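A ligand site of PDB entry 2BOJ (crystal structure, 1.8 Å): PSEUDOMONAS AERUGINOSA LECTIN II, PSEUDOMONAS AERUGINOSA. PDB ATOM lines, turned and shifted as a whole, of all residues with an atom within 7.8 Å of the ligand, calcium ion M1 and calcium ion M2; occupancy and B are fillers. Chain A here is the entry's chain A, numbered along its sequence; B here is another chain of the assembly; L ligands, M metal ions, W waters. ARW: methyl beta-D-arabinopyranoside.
The side-chain carboxylate (OD1) of Asp 96 lies close to an oxygen (O2) of the ligand (2.7 Å). N of Ser 23 sits at hydrogen-bond distance from O5 of the ligand, 2.9 Å away. An oxygen (O5) of the ligand is in hydrogen-bond range of the side-chain hydroxyl of Ser 23 (3.3 Å). OG of Ser 22 sits close to O5 of the ligand, at 3.4 Å.
NE2 of Gln 43 sits at hydrogen-bond distance from O of Ser 22. O of Ser 44 lies within hydrogen-bond range of N of Ser 22 (2.7 Å). The side-chain amide nitrogen (ND2) of Asn 103 is in hydrogen-bond range of the backbone carbonyl oxygen (O) of Pro 112 of chain B, 2.8 Å away. O of Leu 113 of chain B sits close to ND2 of Asn 103 (3.4 Å). OG of Ser 22 sits at hydrogen-bond distance from OD2 of Asp 96. O of Asp 96 lies within hydrogen-bond range of NH2 of Arg 72, at 2.7 Å. O of Ser 44 sits close to N of Asn 21 (3.3 Å). The backbone NH (N) of Asp 104 lies within hydrogen-bond range of the backbone carbonyl oxygen (O) of Ser 94 (3.0 Å).
Merely in contact with the ligand: Gly 97 (3.99 Å). Ten residues have an atom within 4 Å of the ligand: Asn 21, Ser 22, Ser 23, Glu 95, Asp 96, Gly 97, Asp 99, Asp 101, Asp 104 and Gly 114 of chain B.
The nearest printed residue that does not touch calcium ion M1 is Ser 22 (4.3 Å).
Of the 26 residues printed, 4 come within 4 Å of calcium ion M2.
Calcium ion M1 is bound by the side-chain amide oxygen of Asn 103 (2.3 Å), the backbone carbonyl oxygen of Asn 21 (2.3 Å), the side-chain carboxylate of Asp 104 (2.4 Å), an oxygen (O3) of the ligand (2.4 Å), the side-chain carboxylate of Asp 101 (2.4 Å), the chain-end carboxylate of Gly 114 of chain B (2.5 Å) and an oxygen (O4) of the ligand (2.5 Å). Slightly farther from calcium ion M1 lies the side-chain carboxylate (OD1) of Asp 101 (3.1 Å).
Calcium ion M2 is bound by OD1 of Asp 99 (2.3 Å), OD1 of Asp 101 (2.3 Å), OE1 of Glu 95 (2.5 Å), OD2 of Asp 104 (2.5 Å), O2 of the ligand (2.5 Å), O3 of the ligand (2.5 Å), OE2 of Glu 95 (2.5 Å) and OD1 of Asp 104 (2.7 Å). Calcium ion M2 has eight donor atoms within binding distance.
Water W1 lies within hydrogen-bond range of the backbone NH (N) of Thr 98 (2.9 Å), an oxygen (O1) of the ligand (2.9 Å) and the backbone NH (N) of Asp 99 (3.5 Å).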
ATOM      1  N   ALA A  20      11.704  -3.031   2.589  1.00  0.00           N
ATOM      2  CA  ALA A  20      11.381  -1.749   1.939  1.00  0.00           C
ATOM      3  C   ALA A  20      11.536  -1.841   0.442  1.00  0.00           C
ATOM      4  O   ALA A  20      12.474  -2.477  -0.070  1.00  0.00           O
ATOM      5  CB  ALA A  20      12.237  -0.619   2.499  1.00  0.00           C
ATOM      6  N   ASN A  21      10.584  -1.211  -0.265  1.00  0.00           N
ATOM      7  CA  ASN A  21      10.609  -1.121  -1.737  1.00  0.00           C
ATOM      8  C   ASN A  21      10.086   0.249  -2.174  1.00  0.00           C
ATOM      9  O   ASN A  21       8.972   0.356  -2.696  1.00  0.00           O
ATOM     10  CB  ASN A  21       9.776  -2.226  -2.369  1.00  0.00           C
ATOM     11  CG  ASN A  21      10.368  -3.603  -2.168  1.00  0.00           C
ATOM     12  OD1 ASN A  21      11.292  -4.003  -2.866  1.00  0.00           O
ATOM     13  ND2 ASN A  21       9.792  -4.351  -1.228  1.00  0.00           N
ATOM     14  N   SER A  22      10.869   1.297  -1.941  1.00  0.00           N
ATOM     15  CA  SER A  22      10.401   2.647  -2.225  1.00  0.00           C
ATOM     16  C   SER A  22      11.538   3.655  -2.174  1.00  0.00           C
ATOM     17  O   SER A  22      12.563   3.428  -1.534  1.00  0.00           O
ATOM     18  CB  SER A  22       9.336   3.079  -1.194  1.00  0.00           C
ATOM     19  OG  SER A  22       8.897   4.413  -1.452  1.00  0.00           O
ATOM     20  N   SER A  23      11.334   4.802  -2.835  1.00  0.00           N
ATOM     21  CA  SER A  23      12.257   5.920  -2.745  1.00  0.00           C
ATOM     22  C   SER A  23      12.038   6.694  -1.435  1.00  0.00           C
ATOM     23  O   SER A  23      12.860   7.522  -1.036  1.00  0.00           O
ATOM     24  CB  SER A  23      12.097   6.830  -3.961  1.00  0.00           C
ATOM     25  OG  SER A  23      12.298   6.075  -5.138  1.00  0.00           O
ATOM     26  N   GLY A  24      10.920   6.385  -0.781  1.00  0.00           N
ATOM     27  CA  GLY A  24      10.593   6.971   0.507  1.00  0.00           C
ATOM     28  C   GLY A  24      11.168   6.150   1.639  1.00  0.00           C
ATOM     29  O   GLY A  24      11.159   4.896   1.602  1.00  0.00           O
ATOM     30  N   GLN A  26      10.997   4.406   4.976  1.00  0.00           N
ATOM     31  CA  GLN A  26       9.874   3.777   5.659  1.00  0.00           C
ATOM     32  C   GLN A  26      10.097   3.754   7.164  1.00  0.00           C
ATOM     33  O   GLN A  26      11.186   3.407   7.615  1.00  0.00           O
ATOM     34  CB  GLN A  26       9.723   2.325   5.178  1.00  0.00           C
ATOM     35  CG  GLN A  26       9.590   2.174   3.628  1.00  0.00           C
ATOM     36  CD  GLN A  26       8.335   2.826   3.079  1.00  0.00           C
ATOM     37  OE1 GLN A  26       7.227   2.577   3.581  1.00  0.00           O
ATOM     38  NE2 GLN A  26       8.498   3.651   2.030  1.00  0.00           N
ATOM     39  N   GLN A  43      15.552   2.563   3.979  1.00  0.00           N
ATOM     40  CA  GLN A  43      15.151   2.919   2.626  1.00  0.00           C
ATOM     41  C   GLN A  43      15.859   1.955   1.685  1.00  0.00           C
ATOM     42  O   GLN A  43      17.079   1.745   1.772  1.00  0.00           O
ATOM     43  CB  GLN A  43      15.536   4.374   2.341  1.00  0.00           C
ATOM     44  CG  GLN A  43      15.082   4.899   0.976  1.00  0.00           C
ATOM     45  CD  GLN A  43      15.997   4.489  -0.148  1.00  0.00           C
ATOM     46  OE1 GLN A  43      17.223   4.614  -0.051  1.00  0.00           O
ATOM     47  NE2 GLN A  43      15.420   4.025  -1.260  1.00  0.00           N
ATOM     48  N   SER A  44      15.072   1.347   0.811  1.00  0.00           N
ATOM     49  CA  SER A  44      15.560   0.440  -0.221  1.00  0.00           C
ATOM     50  C   SER A  44      14.546   0.386  -1.331  1.00  0.00           C
ATOM     51  O   SER A  44      13.336   0.449  -1.082  1.00  0.00           O
ATOM     52  CB  SER A  44      15.721  -0.954   0.363  1.00  0.00           C
ATOM     53  OG  SER A  44      16.196  -1.876  -0.624  1.00  0.00           O
ATOM     54  N   THR A  45      15.030   0.234  -2.562  1.00  0.00           N
ATOM     55  CA  THR A  45      14.160  -0.108  -3.697  1.00  0.00           C
ATOM     56  C   THR A  45      14.397  -1.570  -4.119  1.00  0.00           C
ATOM     57  O   THR A  45      13.940  -2.016  -5.176  1.00  0.00           O
ATOM     58  CB  THR A  45      14.366   0.847  -4.897  1.00  0.00           C
ATOM     59  OG1 THR A  45      15.763   0.854  -5.242  1.00  0.00           O
ATOM     60  CG2 THR A  45      13.900   2.270  -4.548  1.00  0.00           C
ATOM     61  N   VAL A  69       5.694   7.415   6.068  1.00  0.00           N
ATOM     62  CA  VAL A  69       6.765   7.929   5.252  1.00  0.00           C
ATOM     63  C   VAL A  69       6.619   9.431   5.373  1.00  0.00           C
ATOM     64  O   VAL A  69       5.540   9.980   5.084  1.00  0.00           O
ATOM     65  CB  VAL A  69       6.648   7.433   3.783  1.00  0.00           C
ATOM     66  CG1 VAL A  69       7.862   7.912   2.954  1.00  0.00           C
ATOM     67  CG2 VAL A  69       6.553   5.910   3.736  1.00  0.00           C
ATOM     68  N   ARG A  72       3.593  10.854   7.216  1.00  0.00           N
ATOM     69  CA  ARG A  72       2.282  10.556   6.625  1.00  0.00           C
ATOM     70  C   ARG A  72       2.036   9.058   6.672  1.00  0.00           C
ATOM     71  O   ARG A  72       2.849   8.298   6.177  1.00  0.00           O
ATOM     72  CB  ARG A  72       2.224  10.974   5.166  1.00  0.00           C
ATOM     73  CG  ARG A  72       2.388  12.459   4.813  1.00  0.00           C
ATOM     74  CD  ARG A  72       2.715  12.597   3.317  1.00  0.00           C
ATOM     75  NE  ARG A  72       2.628  11.294   2.644  1.00  0.00           N
ATOM     76  CZ  ARG A  72       3.692  10.542   2.304  1.00  0.00           C
ATOM     77  NH1 ARG A  72       4.924  10.971   2.544  1.00  0.00           N
ATOM     78  NH2 ARG A  72       3.503   9.350   1.727  1.00  0.00           N
ATOM     79  N   SER A  94       1.890  -1.863   2.134  1.00  0.00           N
ATOM     80  CA  SER A  94       1.620  -0.448   2.352  1.00  0.00           C
ATOM     81  C   SER A  94       1.975   0.366   1.126  1.00  0.00           C
ATOM     82  O   SER A  94       2.910   0.012   0.392  1.00  0.00           O
ATOM     83  CB  SER A  94       2.405   0.072   3.569  1.00  0.00           C
ATOM     84  OG  SER A  94       3.799  -0.041   3.358  1.00  0.00           O
ATOM     85  N   GLU A  95       1.230   1.453   0.930  1.00  0.00           N
ATOM     86  CA  GLU A  95       1.413   2.323  -0.230  1.00  0.00           C
ATOM     87  C   GLU A  95       1.670   3.751   0.264  1.00  0.00           C
ATOM     88  O   GLU A  95       0.873   4.305   1.023  1.00  0.00           O
ATOM     89  CB  GLU A  95       0.180   2.270  -1.120  1.00  0.00           C
ATOM     90  CG  GLU A  95       0.245   3.209  -2.324  1.00  0.00           C
ATOM     91  CD  GLU A  95       1.536   3.024  -3.122  1.00  0.00           C
ATOM     92  OE1 GLU A  95       1.892   1.860  -3.447  1.00  0.00           O
ATOM     93  OE2 GLU A  95       2.207   4.047  -3.406  1.00  0.00           O
ATOM     94  N   ASP A  96       2.782   4.331  -0.164  1.00  0.00           N
ATOM     95  CA  ASP A  96       3.177   5.674   0.287  1.00  0.00           C
ATOM     96  C   ASP A  96       3.002   6.738  -0.803  1.00  0.00           C
ATOM     97  O   ASP A  96       3.265   7.931  -0.589  1.00  0.00           O
ATOM     98  CB  ASP A  96       4.630   5.669   0.815  1.00  0.00           C
ATOM     99  CG  ASP A  96       5.681   5.409  -0.269  1.00  0.00           C
ATOM    100  OD1 ASP A  96       5.444   5.725  -1.466  1.00  0.00           O
ATOM    101  OD2 ASP A  96       6.763   4.901   0.090  1.00  0.00           O
ATOM    102  N   GLY A  97       2.540   6.316  -1.975  1.00  0.00           N
ATOM    103  CA  GLY A  97       2.541   7.196  -3.142  1.00  0.00           C
ATOM    104  C   GLY A  97       1.348   6.987  -4.053  1.00  0.00           C
ATOM    105  O   GLY A  97       0.230   6.808  -3.585  1.00  0.00           O
ATOM    106  N   THR A  98       1.609   6.976  -5.357  1.00  0.00           N
ATOM    107  CA  THR A  98       0.572   7.035  -6.368  1.00  0.00           C
ATOM    108  C   THR A  98       0.595   5.859  -7.350  1.00  0.00           C
ATOM    109  O   THR A  98      -0.261   5.797  -8.261  1.00  0.00           O
ATOM    110  CB  THR A  98       0.677   8.342  -7.188  1.00  0.00           C
ATOM    111  OG1 THR A  98       1.995   8.436  -7.736  1.00  0.00           O
ATOM    112  CG2 THR A  98       0.445   9.554  -6.280  1.00  0.00           C
ATOM    113  N   ASP A  99       1.540   4.934  -7.191  1.00  0.00           N
ATOM    114  CA  ASP A  99       1.655   3.839  -8.159  1.00  0.00           C
ATOM    115  C   ASP A  99       0.898   2.563  -7.759  1.00  0.00           C
ATOM    116  O   ASP A  99       0.844   1.606  -8.522  1.00  0.00           O
ATOM    117  CB  ASP A  99       3.119   3.512  -8.470  1.00  0.00           C
ATOM    118  CG  ASP A  99       3.844   2.890  -7.288  1.00  0.00           C
ATOM    119  OD1 ASP A  99       3.404   3.065  -6.125  1.00  0.00           O
ATOM    120  OD2 ASP A  99       4.896   2.250  -7.503  1.00  0.00           O
ATOM    121  N   ASN A 100       0.365   2.561  -6.532  1.00  0.00           N
ATOM    122  CA  ASN A 100      -0.449   1.449  -6.025  1.00  0.00           C
ATOM    123  C   ASN A 100       0.191   0.090  -6.166  1.00  0.00           C
ATOM    124  O   ASN A 100      -0.476  -0.902  -6.476  1.00  0.00           O
ATOM    125  CB  ASN A 100      -1.828   1.457  -6.673  1.00  0.00           C
ATOM    126  CG  ASN A 100      -2.635   2.674  -6.268  1.00  0.00           C
ATOM    127  OD1 ASN A 100      -2.497   3.164  -5.138  1.00  0.00           O
ATOM    128  ND2 ASN A 100      -3.453   3.176  -7.189  1.00  0.00           N
ATOM    129  N   ASP A 101       1.502   0.032  -5.931  1.00  0.00           N
ATOM    130  CA  ASP A 101       2.155  -1.283  -5.844  1.00  0.00           C
ATOM    131  C   ASP A 101       2.049  -1.936  -4.451  1.00  0.00           C
ATOM    132  O   ASP A 101       2.211  -3.149  -4.334  1.00  0.00           O
ATOM    133  CB  ASP A 101       3.595  -1.266  -6.403  1.00  0.00           C
ATOM    134  CG  ASP A 101       4.564  -0.408  -5.596  1.00  0.00           C
ATOM    135  OD1 ASP A 101       4.201   0.339  -4.649  1.00  0.00           O
ATOM    136  OD2 ASP A 101       5.768  -0.495  -5.945  1.00  0.00           O
ATOM    137  N   TYR A 102       1.793  -1.134  -3.397  1.00  0.00           N
ATOM    138  CA  TYR A 102       1.558  -1.648  -2.028  1.00  0.00           C
ATOM    139  C   TYR A 102       2.720  -2.465  -1.422  1.00  0.00           C
ATOM    140  O   TYR A 102       2.538  -3.237  -0.504  1.00  0.00           O
ATOM    141  CB  TYR A 102       0.188  -2.384  -1.910  1.00  0.00           C
ATOM    142  CG  TYR A 102      -0.909  -1.372  -1.809  1.00  0.00           C
ATOM    143  CD1 TYR A 102      -1.333  -0.905  -0.571  1.00  0.00           C
ATOM    144  CD2 TYR A 102      -1.461  -0.791  -2.964  1.00  0.00           C
ATOM    145  CE1 TYR A 102      -2.288   0.078  -0.460  1.00  0.00           C
ATOM    146  CE2 TYR A 102      -2.425   0.202  -2.863  1.00  0.00           C
ATOM    147  CZ  TYR A 102      -2.840   0.626  -1.615  1.00  0.00           C
ATOM    148  OH  TYR A 102      -3.776   1.608  -1.464  1.00  0.00           O
ATOM    149  N   ASN A 103       3.909  -2.233  -1.939  1.00  0.00           N
ATOM    150  CA  ASN A 103       5.078  -2.993  -1.476  1.00  0.00           C
ATOM    151  C   ASN A 103       6.070  -2.055  -0.788  1.00  0.00           C
ATOM    152  O   ASN A 103       7.202  -2.453  -0.474  1.00  0.00           O
ATOM    153  CB  ASN A 103       5.735  -3.703  -2.663  1.00  0.00           C
ATOM    154  CG  ASN A 103       6.533  -2.743  -3.571  1.00  0.00           C
ATOM    155  OD1 ASN A 103       6.490  -1.517  -3.361  1.00  0.00           O
ATOM    156  ND2 ASN A 103       7.257  -3.281  -4.545  1.00  0.00           N
ATOM    157  N   ASP A 104       5.662  -0.807  -0.538  1.00  0.00           N
ATOM    158  CA  ASP A 104       6.627   0.227  -0.134  1.00  0.00           C
ATOM    159  C   ASP A 104       7.268  -0.130   1.193  1.00  0.00           C
ATOM    160  O   ASP A 104       8.481   0.005   1.367  1.00  0.00           O
ATOM    161  CB  ASP A 104       5.954   1.584  -0.102  1.00  0.00           C
ATOM    162  CG  ASP A 104       5.470   2.010  -1.478  1.00  0.00           C
ATOM    163  OD1 ASP A 104       6.112   1.607  -2.473  1.00  0.00           O
ATOM    164  OD2 ASP A 104       4.449   2.694  -1.558  1.00  0.00           O
ATOM    165  N   ALA A 105       6.442  -0.614   2.106  1.00  0.00           N
ATOM    166  CA  ALA A 105       6.935  -1.394   3.238  1.00  0.00           C
ATOM    167  C   ALA A 105       6.085  -2.640   3.268  1.00  0.00           C
ATOM    168  O   ALA A 105       4.845  -2.566   3.204  1.00  0.00           O
ATOM    169  CB  ALA A 105       6.851  -0.637   4.539  1.00  0.00           C
ATOM    170  N   PRO B 112       5.563  -7.780  -6.283  1.00  0.00           N
ATOM    171  CA  PRO B 112       6.742  -7.234  -6.978  1.00  0.00           C
ATOM    172  C   PRO B 112       7.627  -6.446  -6.023  1.00  0.00           C
ATOM    173  O   PRO B 112       7.193  -6.028  -4.938  1.00  0.00           O
ATOM    174  CB  PRO B 112       6.133  -6.285  -7.998  1.00  0.00           C
ATOM    175  CG  PRO B 112       4.878  -5.817  -7.354  1.00  0.00           C
ATOM    176  CD  PRO B 112       4.342  -7.025  -6.620  1.00  0.00           C
ATOM    177  N   LEU B 113       8.854  -6.178  -6.471  1.00  0.00           N
ATOM    178  CA  LEU B 113       9.759  -5.311  -5.735  1.00  0.00           C
ATOM    179  C   LEU B 113       9.827  -3.941  -6.412  1.00  0.00           C
ATOM    180  O   LEU B 113       9.126  -3.696  -7.399  1.00  0.00           O
ATOM    181  CB  LEU B 113      11.142  -5.947  -5.661  1.00  0.00           C
ATOM    182  CG  LEU B 113      11.194  -7.420  -5.238  1.00  0.00           C
ATOM    183  CD1 LEU B 113      12.662  -7.868  -5.247  1.00  0.00           C
ATOM    184  CD2 LEU B 113      10.500  -7.664  -3.891  1.00  0.00           C
ATOM    185  N   GLY B 114      10.629  -3.038  -5.838  1.00  0.00           N
ATOM    186  CA  GLY B 114      10.905  -1.752  -6.480  1.00  0.00           C
ATOM    187  C   GLY B 114      10.002  -0.630  -5.984  1.00  0.00           C
ATOM    188  O   GLY B 114       8.881  -0.867  -5.515  1.00  0.00           O
ATOM    189  OXT GLY B 114      10.399   0.541  -6.068  1.00  0.00           O
HETATM  190  C1  ARW L   1       7.847   5.523  -4.381  1.00  0.00           C
HETATM  191  C2  ARW L   1       6.950   4.284  -4.274  1.00  0.00           C
HETATM  192  C3  ARW L   1       6.962   3.548  -5.611  1.00  0.00           C
HETATM  193  C4  ARW L   1       8.379   3.177  -6.017  1.00  0.00           C
HETATM  194  C5  ARW L   1       9.346   4.365  -5.955  1.00  0.00           C
HETATM  195  O1  ARW L   1       7.234   6.401  -5.338  1.00  0.00           O
HETATM  196  O2  ARW L   1       5.606   4.623  -3.879  1.00  0.00           O
HETATM  197  O3  ARW L   1       6.209   2.328  -5.455  1.00  0.00           O
HETATM  198  O4  ARW L   1       8.863   2.184  -5.095  1.00  0.00           O
HETATM  199  O5  ARW L   1       9.178   5.089  -4.724  1.00  0.00           O
HETATM  200  CM  ARW L   1       7.859   7.692  -5.410  1.00  0.00           C
HETATM  201 CA    CA M   1       7.237   0.477  -4.261  1.00  0.00          CA
HETATM  202 CA    CA M   2       4.159   2.589  -4.033  1.00  0.00          CA
HETATM  203  O   HOH W   1       4.379   6.541  -6.025  1.00  0.00           O
HETATM  204  O   HOH W   2       5.011   9.435  -4.569  1.00  0.00           O
